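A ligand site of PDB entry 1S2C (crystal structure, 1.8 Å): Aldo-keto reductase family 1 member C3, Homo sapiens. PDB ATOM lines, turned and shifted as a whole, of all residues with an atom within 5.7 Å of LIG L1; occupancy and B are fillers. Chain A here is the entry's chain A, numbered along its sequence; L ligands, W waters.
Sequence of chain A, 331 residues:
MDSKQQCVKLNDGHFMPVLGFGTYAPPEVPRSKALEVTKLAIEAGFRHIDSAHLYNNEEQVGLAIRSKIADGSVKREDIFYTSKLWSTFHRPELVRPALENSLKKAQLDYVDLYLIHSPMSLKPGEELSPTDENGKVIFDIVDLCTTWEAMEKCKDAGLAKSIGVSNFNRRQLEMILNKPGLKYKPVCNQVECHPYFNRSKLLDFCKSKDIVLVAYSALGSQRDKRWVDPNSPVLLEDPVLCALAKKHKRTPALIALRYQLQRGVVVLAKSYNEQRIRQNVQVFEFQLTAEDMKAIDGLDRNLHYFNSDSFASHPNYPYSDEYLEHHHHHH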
ATOM      1  N   TYR A  24      18.179   8.498 -15.680  1.00  0.00           N
ATOM      2  CA  TYR A  24      18.047   9.581 -14.699  1.00  0.00           C
ATOM      3  C   TYR A  24      16.865  10.490 -15.021  1.00  0.00           C
ATOM      4  O   TYR A  24      16.713  10.965 -16.155  1.00  0.00           O
ATOM      5  CB  TYR A  24      19.299  10.445 -14.588  1.00  0.00           C
ATOM      6  CG  TYR A  24      19.126  11.515 -13.527  1.00  0.00           C
ATOM      7  CD1 TYR A  24      19.200  11.195 -12.183  1.00  0.00           C
ATOM      8  CD2 TYR A  24      18.814  12.831 -13.871  1.00  0.00           C
ATOM      9  CE1 TYR A  24      19.006  12.151 -11.199  1.00  0.00           C
ATOM     10  CE2 TYR A  24      18.617  13.805 -12.878  1.00  0.00           C
ATOM     11  CZ  TYR A  24      18.728  13.457 -11.555  1.00  0.00           C
ATOM     12  OH  TYR A  24      18.544  14.383 -10.551  1.00  0.00           O
ATOM     13  N   ALA A  52      22.407   4.250 -11.696  1.00  0.00           N
ATOM     14  CA  ALA A  52      23.401   4.637 -10.697  1.00  0.00           C
ATOM     15  C   ALA A  52      22.764   4.714  -9.319  1.00  0.00           C
ATOM     16  O   ALA A  52      21.564   4.963  -9.211  1.00  0.00           O
ATOM     17  CB  ALA A  52      24.008   5.988 -11.041  1.00  0.00           C
ATOM     18  N   LEU A  54      23.146   7.152  -7.358  1.00  0.00           N
ATOM     19  CA  LEU A  54      22.729   8.556  -7.295  1.00  0.00           C
ATOM     20  C   LEU A  54      21.292   8.781  -7.784  1.00  0.00           C
ATOM     21  O   LEU A  54      20.602   9.697  -7.312  1.00  0.00           O
ATOM     22  CB  LEU A  54      23.697   9.403  -8.124  1.00  0.00           C
ATOM     23  CG  LEU A  54      23.424  10.912  -8.193  1.00  0.00           C
ATOM     24  CD1 LEU A  54      23.646  11.523  -6.823  1.00  0.00           C
ATOM     25  CD2 LEU A  54      24.291  11.574  -9.272  1.00  0.00           C
ATOM     26  N   TYR A  55      20.847   7.967  -8.733  1.00  0.00           N
ATOM     27  CA  TYR A  55      19.581   8.221  -9.420  1.00  0.00           C
ATOM     28  C   TYR A  55      18.345   7.849  -8.617  1.00  0.00           C
ATOM     29  O   TYR A  55      17.241   8.220  -9.005  1.00  0.00           O
ATOM     30  CB  TYR A  55      19.553   7.496 -10.774  1.00  0.00           C
ATOM     31  CG  TYR A  55      20.714   7.833 -11.703  1.00  0.00           C
ATOM     32  CD1 TYR A  55      20.893   7.110 -12.874  1.00  0.00           C
ATOM     33  CD2 TYR A  55      21.603   8.870 -11.428  1.00  0.00           C
ATOM     34  CE1 TYR A  55      21.945   7.382 -13.739  1.00  0.00           C
ATOM     35  CE2 TYR A  55      22.662   9.145 -12.272  1.00  0.00           C
ATOM     36  CZ  TYR A  55      22.829   8.412 -13.427  1.00  0.00           C
ATOM     37  OH  TYR A  55      23.882   8.699 -14.276  1.00  0.00           O
ATOM     38  N   LYS A  84      26.619   2.578 -10.876  1.00  0.00           N
ATOM     39  CA  LYS A  84      27.788   3.382 -10.580  1.00  0.00           C
ATOM     40  C   LYS A  84      27.961   3.604  -9.078  1.00  0.00           C
ATOM     41  O   LYS A  84      26.992   3.832  -8.350  1.00  0.00           O
ATOM     42  CB  LYS A  84      27.702   4.736 -11.283  1.00  0.00           C
ATOM     43  CG  LYS A  84      27.225   4.684 -12.731  1.00  0.00           C
ATOM     44  CD  LYS A  84      27.330   6.053 -13.382  1.00  0.00           C
ATOM     45  CE  LYS A  84      26.755   6.076 -14.770  1.00  0.00           C
ATOM     46  NZ  LYS A  84      25.282   6.034 -14.764  1.00  0.00           N
ATOM     47  N   TRP A  86      28.787   5.712  -6.087  1.00  0.00           N
ATOM     48  CA  TRP A  86      28.692   7.117  -5.764  1.00  0.00           C
ATOM     49  C   TRP A  86      29.938   7.594  -4.987  1.00  0.00           C
ATOM     50  O   TRP A  86      30.628   6.809  -4.336  1.00  0.00           O
ATOM     51  CB  TRP A  86      27.376   7.467  -5.045  1.00  0.00           C
ATOM     52  CG  TRP A  86      27.247   8.950  -4.806  1.00  0.00           C
ATOM     53  CD1 TRP A  86      27.057   9.582  -3.613  1.00  0.00           C
ATOM     54  CD2 TRP A  86      27.392   9.982  -5.795  1.00  0.00           C
ATOM     55  NE1 TRP A  86      27.049  10.945  -3.803  1.00  0.00           N
ATOM     56  CE2 TRP A  86      27.263  11.214  -5.125  1.00  0.00           C
ATOM     57  CE3 TRP A  86      27.644   9.992  -7.171  1.00  0.00           C
ATOM     58  CZ2 TRP A  86      27.348  12.450  -5.788  1.00  0.00           C
ATOM     59  CZ3 TRP A  86      27.716  11.203  -7.835  1.00  0.00           C
ATOM     60  CH2 TRP A  86      27.583  12.419  -7.134  1.00  0.00           C
ATOM     61  N   SER A  87      30.187   8.902  -5.067  1.00  0.00           N
ATOM     62  CA  SER A  87      31.451   9.497  -4.646  1.00  0.00           C
ATOM     63  C   SER A  87      31.705   9.506  -3.134  1.00  0.00           C
ATOM     64  O   SER A  87      32.835   9.731  -2.706  1.00  0.00           O
ATOM     65  CB  SER A  87      31.527  10.903  -5.220  1.00  0.00           C
ATOM     66  OG  SER A  87      31.374  10.867  -6.632  1.00  0.00           O
ATOM     67  N   HIS A 117      31.500   6.658 -10.496  1.00  0.00           N
ATOM     68  CA  HIS A 117      30.632   7.713 -11.057  1.00  0.00           C
ATOM     69  C   HIS A 117      31.399   8.986 -11.402  1.00  0.00           C
ATOM     70  O   HIS A 117      31.108   9.658 -12.397  1.00  0.00           O
ATOM     71  CB  HIS A 117      29.523   8.069 -10.069  1.00  0.00           C
ATOM     72  CG  HIS A 117      28.302   8.650 -10.714  1.00  0.00           C
ATOM     73  ND1 HIS A 117      27.035   8.227 -10.383  1.00  0.00           N
ATOM     74  CD2 HIS A 117      28.148   9.616 -11.649  1.00  0.00           C
ATOM     75  CE1 HIS A 117      26.141   8.900 -11.101  1.00  0.00           C
ATOM     76  NE2 HIS A 117      26.793   9.746 -11.880  1.00  0.00           N
ATOM     77  N   SER A 118      32.363   9.322 -10.548  1.00  0.00           N
ATOM     78  CA  SER A 118      33.085  10.593 -10.649  1.00  0.00           C
ATOM     79  C   SER A 118      34.399  10.504  -9.883  1.00  0.00           C
ATOM     80  O   SER A 118      34.476   9.801  -8.871  1.00  0.00           O
ATOM     81  CB  SER A 118      32.197  11.717 -10.086  1.00  0.00           C
ATOM     82  OG  SER A 118      32.949  12.846  -9.686  1.00  0.00           O
ATOM     83  N   PRO A 119      35.451  11.194 -10.346  1.00  0.00           N
ATOM     84  CA  PRO A 119      36.721  11.217  -9.600  1.00  0.00           C
ATOM     85  C   PRO A 119      36.699  12.160  -8.394  1.00  0.00           C
ATOM     86  O   PRO A 119      37.666  12.193  -7.637  1.00  0.00           O
ATOM     87  CB  PRO A 119      37.713  11.722 -10.649  1.00  0.00           C
ATOM     88  CG  PRO A 119      36.911  12.609 -11.514  1.00  0.00           C
ATOM     89  CD  PRO A 119      35.545  11.974 -11.588  1.00  0.00           C
ATOM     90  N   MET A 120      35.600  12.890  -8.210  1.00  0.00           N
ATOM     91  CA  MET A 120      35.523  13.918  -7.184  1.00  0.00           C
ATOM     92  C   MET A 120      34.983  13.311  -5.888  1.00  0.00           C
ATOM     93  O   MET A 120      33.791  13.388  -5.604  1.00  0.00           O
ATOM     94  CB  MET A 120      34.646  15.070  -7.669  1.00  0.00           C
ATOM     95  CG  MET A 120      35.299  15.920  -8.738  1.00  0.00           C
ATOM     96  SD  MET A 120      34.176  17.176  -9.479  1.00  0.00           S
ATOM     97  CE  MET A 120      33.140  16.157 -10.400  1.00  0.00           C
ATOM     98  N   ASN A 167      33.494  10.350 -15.895  1.00  0.00           N
ATOM     99  CA  ASN A 167      33.918  11.717 -15.621  1.00  0.00           C
ATOM    100  C   ASN A 167      35.424  11.866 -15.341  1.00  0.00           C
ATOM    101  O   ASN A 167      35.849  12.859 -14.752  1.00  0.00           O
ATOM    102  CB  ASN A 167      33.071  12.320 -14.491  1.00  0.00           C
ATOM    103  CG  ASN A 167      31.619  12.485 -14.884  1.00  0.00           C
ATOM    104  OD1 ASN A 167      31.305  13.138 -15.873  1.00  0.00           O
ATOM    105  ND2 ASN A 167      30.719  11.846 -14.129  1.00  0.00           N
ATOM    106  N   GLU A 192      30.673  13.451 -20.427  1.00  0.00           N
ATOM    107  CA  GLU A 192      29.800  14.370 -21.154  1.00  0.00           C
ATOM    108  C   GLU A 192      30.365  14.509 -22.545  1.00  0.00           C
ATOM    109  O   GLU A 192      31.554  14.808 -22.719  1.00  0.00           O
ATOM    110  CB  GLU A 192      29.702  15.746 -20.488  1.00  0.00           C
ATOM    111  CG  GLU A 192      28.707  16.619 -21.221  1.00  0.00           C
ATOM    112  CD  GLU A 192      28.364  17.942 -20.553  1.00  0.00           C
ATOM    113  OE1 GLU A 192      28.558  18.108 -19.324  1.00  0.00           O
ATOM    114  OE2 GLU A 192      27.896  18.821 -21.300  1.00  0.00           O
ATOM    115  N   TYR A 216      27.413  10.752 -22.468  1.00  0.00           N
ATOM    116  CA  TYR A 216      26.205  11.191 -21.792  1.00  0.00           C
ATOM    117  C   TYR A 216      25.920  12.653 -22.123  1.00  0.00           C
ATOM    118  O   TYR A 216      26.785  13.372 -22.612  1.00  0.00           O
ATOM    119  CB  TYR A 216      26.276  10.945 -20.275  1.00  0.00           C
ATOM    120  CG  TYR A 216      27.107  11.875 -19.400  1.00  0.00           C
ATOM    121  CD1 TYR A 216      28.206  11.397 -18.695  1.00  0.00           C
ATOM    122  CD2 TYR A 216      26.766  13.218 -19.221  1.00  0.00           C
ATOM    123  CE1 TYR A 216      28.950  12.224 -17.854  1.00  0.00           C
ATOM    124  CE2 TYR A 216      27.496  14.043 -18.384  1.00  0.00           C
ATOM    125  CZ  TYR A 216      28.583  13.556 -17.688  1.00  0.00           C
ATOM    126  OH  TYR A 216      29.302  14.396 -16.864  1.00  0.00           O
ATOM    127  N   ARG A 226      19.982  23.138 -11.206  1.00  0.00           N
ATOM    128  CA  ARG A 226      20.946  22.935 -10.144  1.00  0.00           C
ATOM    129  C   ARG A 226      22.385  23.016 -10.649  1.00  0.00           C
ATOM    130  O   ARG A 226      23.267  23.475  -9.922  1.00  0.00           O
ATOM    131  CB  ARG A 226      20.690  21.604  -9.428  1.00  0.00           C
ATOM    132  CG  ARG A 226      19.528  21.668  -8.440  1.00  0.00           C
ATOM    133  CD  ARG A 226      19.180  20.333  -7.805  1.00  0.00           C
ATOM    134  NE  ARG A 226      18.647  19.392  -8.784  1.00  0.00           N
ATOM    135  CZ  ARG A 226      18.547  18.072  -8.614  1.00  0.00           C
ATOM    136  NH1 ARG A 226      18.059  17.314  -9.580  1.00  0.00           N
ATOM    137  NH2 ARG A 226      18.941  17.498  -7.474  1.00  0.00           N
ATOM    138  N   TRP A 227      22.611  22.583 -11.889  1.00  0.00           N
ATOM    139  CA  TRP A 227      23.963  22.488 -12.442  1.00  0.00           C
ATOM    140  C   TRP A 227      24.169  23.142 -13.817  1.00  0.00           C
ATOM    141  O   TRP A 227      25.310  23.330 -14.207  1.00  0.00           O
ATOM    142  CB  TRP A 227      24.383  21.027 -12.527  1.00  0.00           C
ATOM    143  CG  TRP A 227      24.107  20.287 -11.262  1.00  0.00           C
ATOM    144  CD1 TRP A 227      24.764  20.422 -10.072  1.00  0.00           C
ATOM    145  CD2 TRP A 227      23.071  19.326 -11.050  1.00  0.00           C
ATOM    146  NE1 TRP A 227      24.200  19.585  -9.134  1.00  0.00           N
ATOM    147  CE2 TRP A 227      23.163  18.907  -9.704  1.00  0.00           C
ATOM    148  CE3 TRP A 227      22.076  18.763 -11.869  1.00  0.00           C
ATOM    149  CZ2 TRP A 227      22.290  17.956  -9.159  1.00  0.00           C
ATOM    150  CZ3 TRP A 227      21.222  17.826 -11.319  1.00  0.00           C
ATOM    151  CH2 TRP A 227      21.339  17.426  -9.980  1.00  0.00           C
ATOM    152  N   PHE A 306      27.036  20.540 -17.457  1.00  0.00           N
ATOM    153  CA  PHE A 306      27.244  20.448 -16.014  1.00  0.00           C
ATOM    154  C   PHE A 306      28.365  21.420 -15.642  1.00  0.00           C
ATOM    155  O   PHE A 306      29.530  21.172 -15.911  1.00  0.00           O
ATOM    156  CB  PHE A 306      27.598  19.018 -15.602  1.00  0.00           C
ATOM    157  CG  PHE A 306      26.431  18.059 -15.664  1.00  0.00           C
ATOM    158  CD1 PHE A 306      26.049  17.487 -16.879  1.00  0.00           C
ATOM    159  CD2 PHE A 306      25.724  17.733 -14.510  1.00  0.00           C
ATOM    160  CE1 PHE A 306      24.983  16.593 -16.940  1.00  0.00           C
ATOM    161  CE2 PHE A 306      24.651  16.826 -14.572  1.00  0.00           C
ATOM    162  CZ  PHE A 306      24.285  16.271 -15.790  1.00  0.00           C
ATOM    163  N   PHE A 311      30.929  21.594  -8.445  1.00  0.00           N
ATOM    164  CA  PHE A 311      31.886  20.737  -9.135  1.00  0.00           C
ATOM    165  C   PHE A 311      33.251  21.423  -9.310  1.00  0.00           C
ATOM    166  O   PHE A 311      34.304  20.843  -9.026  1.00  0.00           O
ATOM    167  CB  PHE A 311      31.378  20.337 -10.531  1.00  0.00           C
ATOM    168  CG  PHE A 311      30.049  19.639 -10.527  1.00  0.00           C
ATOM    169  CD1 PHE A 311      29.037  20.052 -11.389  1.00  0.00           C
ATOM    170  CD2 PHE A 311      29.795  18.559  -9.674  1.00  0.00           C
ATOM    171  CE1 PHE A 311      27.806  19.414 -11.397  1.00  0.00           C
ATOM    172  CE2 PHE A 311      28.564  17.921  -9.682  1.00  0.00           C
ATOM    173  CZ  PHE A 311      27.572  18.347 -10.539  1.00  0.00           C
ATOM    174  N   TYR A 317      38.247  17.968  -9.796  1.00  0.00           N
ATOM    175  CA  TYR A 317      37.431  18.430 -10.912  1.00  0.00           C
ATOM    176  C   TYR A 317      38.139  18.095 -12.240  1.00  0.00           C
ATOM    177  O   TYR A 317      39.282  18.491 -12.425  1.00  0.00           O
ATOM    178  CB  TYR A 317      37.246  19.939 -10.777  1.00  0.00           C
ATOM    179  CG  TYR A 317      36.375  20.605 -11.801  1.00  0.00           C
ATOM    180  CD1 TYR A 317      35.049  20.210 -11.982  1.00  0.00           C
ATOM    181  CD2 TYR A 317      36.852  21.665 -12.561  1.00  0.00           C
ATOM    182  CE1 TYR A 317      34.233  20.849 -12.902  1.00  0.00           C
ATOM    183  CE2 TYR A 317      36.043  22.317 -13.480  1.00  0.00           C
ATOM    184  CZ  TYR A 317      34.742  21.908 -13.644  1.00  0.00           C
ATOM    185  OH  TYR A 317      33.942  22.539 -14.564  1.00  0.00           O
ATOM    186  N   PRO A 318      37.473  17.350 -13.122  1.00  0.00           N
ATOM    187  CA  PRO A 318      38.125  16.880 -14.356  1.00  0.00           C
ATOM    188  C   PRO A 318      38.376  17.932 -15.435  1.00  0.00           C
ATOM    189  O   PRO A 318      39.247  17.689 -16.269  1.00  0.00           O
ATOM    190  CB  PRO A 318      37.147  15.814 -14.893  1.00  0.00           C
ATOM    191  CG  PRO A 318      35.822  16.201 -14.349  1.00  0.00           C
ATOM    192  CD  PRO A 318      36.090  16.861 -13.013  1.00  0.00           C
ATOM    193  N   TYR A 319      37.651  19.045 -15.417  1.00  0.00           N
ATOM    194  CA  TYR A 319      37.750  20.034 -16.503  1.00  0.00           C
ATOM    195  C   TYR A 319      38.757  21.134 -16.189  1.00  0.00           C
ATOM    196  O   TYR A 319      38.906  21.552 -15.039  1.00  0.00           O
ATOM    197  CB  TYR A 319      36.364  20.641 -16.801  1.00  0.00           C
ATOM    198  CG  TYR A 319      35.282  19.632 -17.148  1.00  0.00           C
ATOM    199  CD1 TYR A 319      35.544  18.577 -18.013  1.00  0.00           C
ATOM    200  CD2 TYR A 319      33.996  19.741 -16.617  1.00  0.00           C
ATOM    201  CE1 TYR A 319      34.562  17.658 -18.338  1.00  0.00           C
ATOM    202  CE2 TYR A 319      32.997  18.814 -16.934  1.00  0.00           C
ATOM    203  CZ  TYR A 319      33.292  17.782 -17.810  1.00  0.00           C
ATOM    204  OH  TYR A 319      32.330  16.852 -18.150  1.00  0.00           O
HETATM  205  C1  LIG L   1      23.797  12.980 -12.888  1.00  0.00           C
HETATM  206  O1  LIG L   1      24.785  10.946 -13.531  1.00  0.00           O
HETATM  207  C2  LIG L   1      22.534  13.463 -12.540  1.00  0.00           C
HETATM  208  C3  LIG L   1      22.437  14.591 -11.733  1.00  0.00           C
HETATM  209  O2  LIG L   1      22.969  11.586 -14.632  1.00  0.00           O
HETATM  210  C4  LIG L   1      23.581  15.233 -11.274  1.00  0.00           C
HETATM  211  C5  LIG L   1      24.866  14.803 -11.604  1.00  0.00           C
HETATM  212  C6  LIG L   1      25.039  13.682 -12.417  1.00  0.00           C
HETATM  213  C7  LIG L   1      23.859  11.761 -13.756  1.00  0.00           C
HETATM  214  N1  LIG L   1      26.277  13.228 -12.741  1.00  0.00           N
HETATM  215  C8  LIG L   1      27.436  13.740 -12.240  1.00  0.00           C
HETATM  216  C9  LIG L   1      28.311  14.490 -13.026  1.00  0.00           C
HETATM  217  C10 LIG L   1      29.509  14.979 -12.484  1.00  0.00           C
HETATM  218  C11 LIG L   1      29.818  14.693 -11.156  1.00  0.00           C
HETATM  219  C12 LIG L   1      28.958  13.934 -10.369  1.00  0.00           C
HETATM  220  C13 LIG L   1      27.769  13.449 -10.916  1.00  0.00           C
HETATM  221  C14 LIG L   1      30.501  15.811 -13.272  1.00  0.00           C
HETATM  222  F1  LIG L   1      30.093  15.954 -14.509  1.00  0.00           F
HETATM  223  F2  LIG L   1      31.672  15.196 -13.288  1.00  0.00           F
HETATM  224  F3  LIG L   1      30.656  17.007 -12.733  1.00  0.00           F
HETATM  225  P1  LG2 L   2      20.162  13.394 -22.666  1.00  0.00           P
HETATM  226  O1  LG2 L   2      21.170  14.366 -23.148  1.00  0.00           O
HETATM  227  O2  LG2 L   2      20.301  11.967 -23.205  1.00  0.00           O
HETATM  228  O3  LG2 L   2      18.686  13.868 -23.032  1.00  0.00           O
HETATM  229  C1  LG2 L   2      18.298  15.201 -22.782  1.00  0.00           C
HETATM  230  C2  LG2 L   2      16.817  15.362 -23.086  1.00  0.00           C
HETATM  231  O4  LG2 L   2      16.551  15.047 -24.434  1.00  0.00           O
HETATM  232  C3  LG2 L   2      15.932  14.438 -22.271  1.00  0.00           C
HETATM  233  O5  LG2 L   2      15.517  15.029 -21.046  1.00  0.00           O
HETATM  234  C4  LG2 L   2      14.778  14.111 -23.205  1.00  0.00           C
HETATM  235  O6  LG2 L   2      13.553  14.656 -22.760  1.00  0.00           O
HETATM  236  C5  LG2 L   2      15.173  14.717 -24.538  1.00  0.00           C
HETATM  237  N1  LG2 L   2      15.016  13.821 -25.708  1.00  0.00           N
HETATM  238  C6  LG2 L   2      15.328  12.489 -25.757  1.00  0.00           C
HETATM  239  N2  LG2 L   2      15.076  12.057 -26.997  1.00  0.00           N
HETATM  240  C7  LG2 L   2      14.623  13.097 -27.744  1.00  0.00           C
HETATM  241  C8  LG2 L   2      14.218  13.193 -29.072  1.00  0.00           C
HETATM  242  N3  LG2 L   2      14.172  12.117 -29.862  1.00  0.00           N
HETATM  243  N4  LG2 L   2      13.787  14.418 -29.536  1.00  0.00           N
HETATM  244  C9  LG2 L   2      13.766  15.529 -28.706  1.00  0.00           C
HETATM  245  N5  LG2 L   2      14.168  15.426 -27.391  1.00  0.00           N
HETATM  246  C10 LG2 L   2      14.590  14.222 -26.927  1.00  0.00           C
HETATM  247  O7  LG2 L   2      19.990  13.372 -21.062  1.00  0.00           O
HETATM  248  P2  LG2 L   2      21.040  13.126 -19.872  1.00  0.00           P
HETATM  249  O8  LG2 L   2      20.257  12.648 -18.717  1.00  0.00           O
HETATM  250  O9  LG2 L   2      21.888  14.326 -19.697  1.00  0.00           O
HETATM  251  O10 LG2 L   2      21.998  11.939 -20.390  1.00  0.00           O
HETATM  252  C11 LG2 L   2      21.429  10.671 -20.606  1.00  0.00           C
HETATM  253  C12 LG2 L   2      21.844   9.648 -19.553  1.00  0.00           C
HETATM  254  O11 LG2 L   2      23.258   9.586 -19.392  1.00  0.00           O
HETATM  255  C13 LG2 L   2      21.290   9.881 -18.157  1.00  0.00           C
HETATM  256  O12 LG2 L   2      19.910   9.605 -17.974  1.00  0.00           O
HETATM  257  C14 LG2 L   2      22.232   8.994 -17.373  1.00  0.00           C
HETATM  258  O13 LG2 L   2      21.831   7.664 -17.503  1.00  0.00           O
HETATM  259  C15 LG2 L   2      23.570   9.233 -18.066  1.00  0.00           C
HETATM  260  N6  LG2 L   2      24.329  10.334 -17.438  1.00  0.00           N
HETATM  261  C16 LG2 L   2      25.440  10.026 -16.729  1.00  0.00           C
HETATM  262  C17 LG2 L   2      26.177  11.026 -16.113  1.00  0.00           C
HETATM  263  C18 LG2 L   2      27.447  10.682 -15.424  1.00  0.00           C
HETATM  264  O14 LG2 L   2      27.931  11.614 -14.515  1.00  0.00           O
HETATM  265  N7  LG2 L   2      28.105   9.534 -15.681  1.00  0.00           N
HETATM  266  C19 LG2 L   2      25.776  12.356 -16.218  1.00  0.00           C
HETATM  267  C20 LG2 L   2      24.644  12.660 -16.953  1.00  0.00           C
HETATM  268  C21 LG2 L   2      23.927  11.649 -17.560  1.00  0.00           C
HETATM  269  P3  LG2 L   2      12.249  13.716 -22.663  1.00  0.00           P
HETATM  270  O15 LG2 L   2      12.451  12.788 -21.525  1.00  0.00           O
HETATM  271  O16 LG2 L   2      11.080  14.698 -22.398  1.00  0.00           O
HETATM  272  O17 LG2 L   2      12.091  12.947 -23.957  1.00  0.00           O
HETATM  273  O   HOH W   1      21.456  13.456 -16.005  1.00  0.00           O
HETATM  274  O   HOH W   2      29.891  17.110 -17.259  1.00  0.00           O
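An oxygen (O1) of LIG L1 lies within hydrogen-bond range of the side-chain hydroxyl (OH) of Tyr 55. NE2 of His 117 sits at hydrogen-bond distance from O1 of LIG L1 (2.9 Å). An oxygen (O14) of LG2 L2 sits at hydrogen-bond distance from a ring nitrogen (NE2) of His 117. ND2 of Asn 167 lies within hydrogen-bond range of O14 of LG2 L2. N of Tyr 24 is in hydrogen-bond range of O12 of LG2 L2, at 3.1 Å.
OD1 of Asn 167 sits close to F2 of LIG L1 (3.3 Å). The side-chain hydroxyl (OH) of Tyr 216 sits close to a fluorine (F1) of LIG L1 (2.9 Å). Tyr 24 touches LIG L1 (CB to O2, 3.8 Å). Leu 54 touches LIG L1. Trp 86 touches LIG L1 (CZ3 to C13, 3.8 Å). OG of Ser 118 touches C11 of LIG L1, at 3.9 Å. CE of Met 120 touches F2 of LIG L1, at 3.4 Å. CH2 of Trp 227 touches C4 of LIG L1 (3.4 Å). Phe 306 touches LIG L1. Phe 311 touches LIG L1 (CG to F3, 3.5 Å). Of the 21 residues printed, 12 come within 4 Å of LIG L1.
Water W1 bridges an oxygen (O2) of LIG L1 (2.8 Å) and an oxygen (O8) of LG2 L2 (3.1 Å). Water W2 lies within hydrogen-bond range of the side-chain hydroxyl (OH) of Tyr 319 (2.6 Å), the side-chain carboxylate (OE1) of Glu 192 (2.7 Å) and the side-chain hydroxyl (OH) of Tyr 216 (2.8 Å).
N1 of LIG L1 lies within hydrogen-bond range of O14 of LG2 L2, 2.9 Å away.
OH of Tyr 55 lies within hydrogen-bond range of NZ of Lys 84, at 3.0 Å. The backbone carbonyl oxygen of His 117 lies within hydrogen-bond range of the side-chain amide nitrogen of Asn 167, 2.8 Å away. OD1 of Asn 167 is in hydrogen-bond range of OH of Tyr 216. The backbone NH (N) of Met 120 lies within hydrogen-bond range of the side-chain hydroxyl (OG) of Ser 118, at 3.0 Å. The backbone NH (N) of Phe 306 sits at hydrogen-bond distance from the side-chain carboxylate (OE1) of Glu 192 (3.4 Å). The side-chain hydroxyl (OH) of Tyr 24 lies within hydrogen-bond range of the guanidinium group (NH1) of Arg 226, 3.1 Å away.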
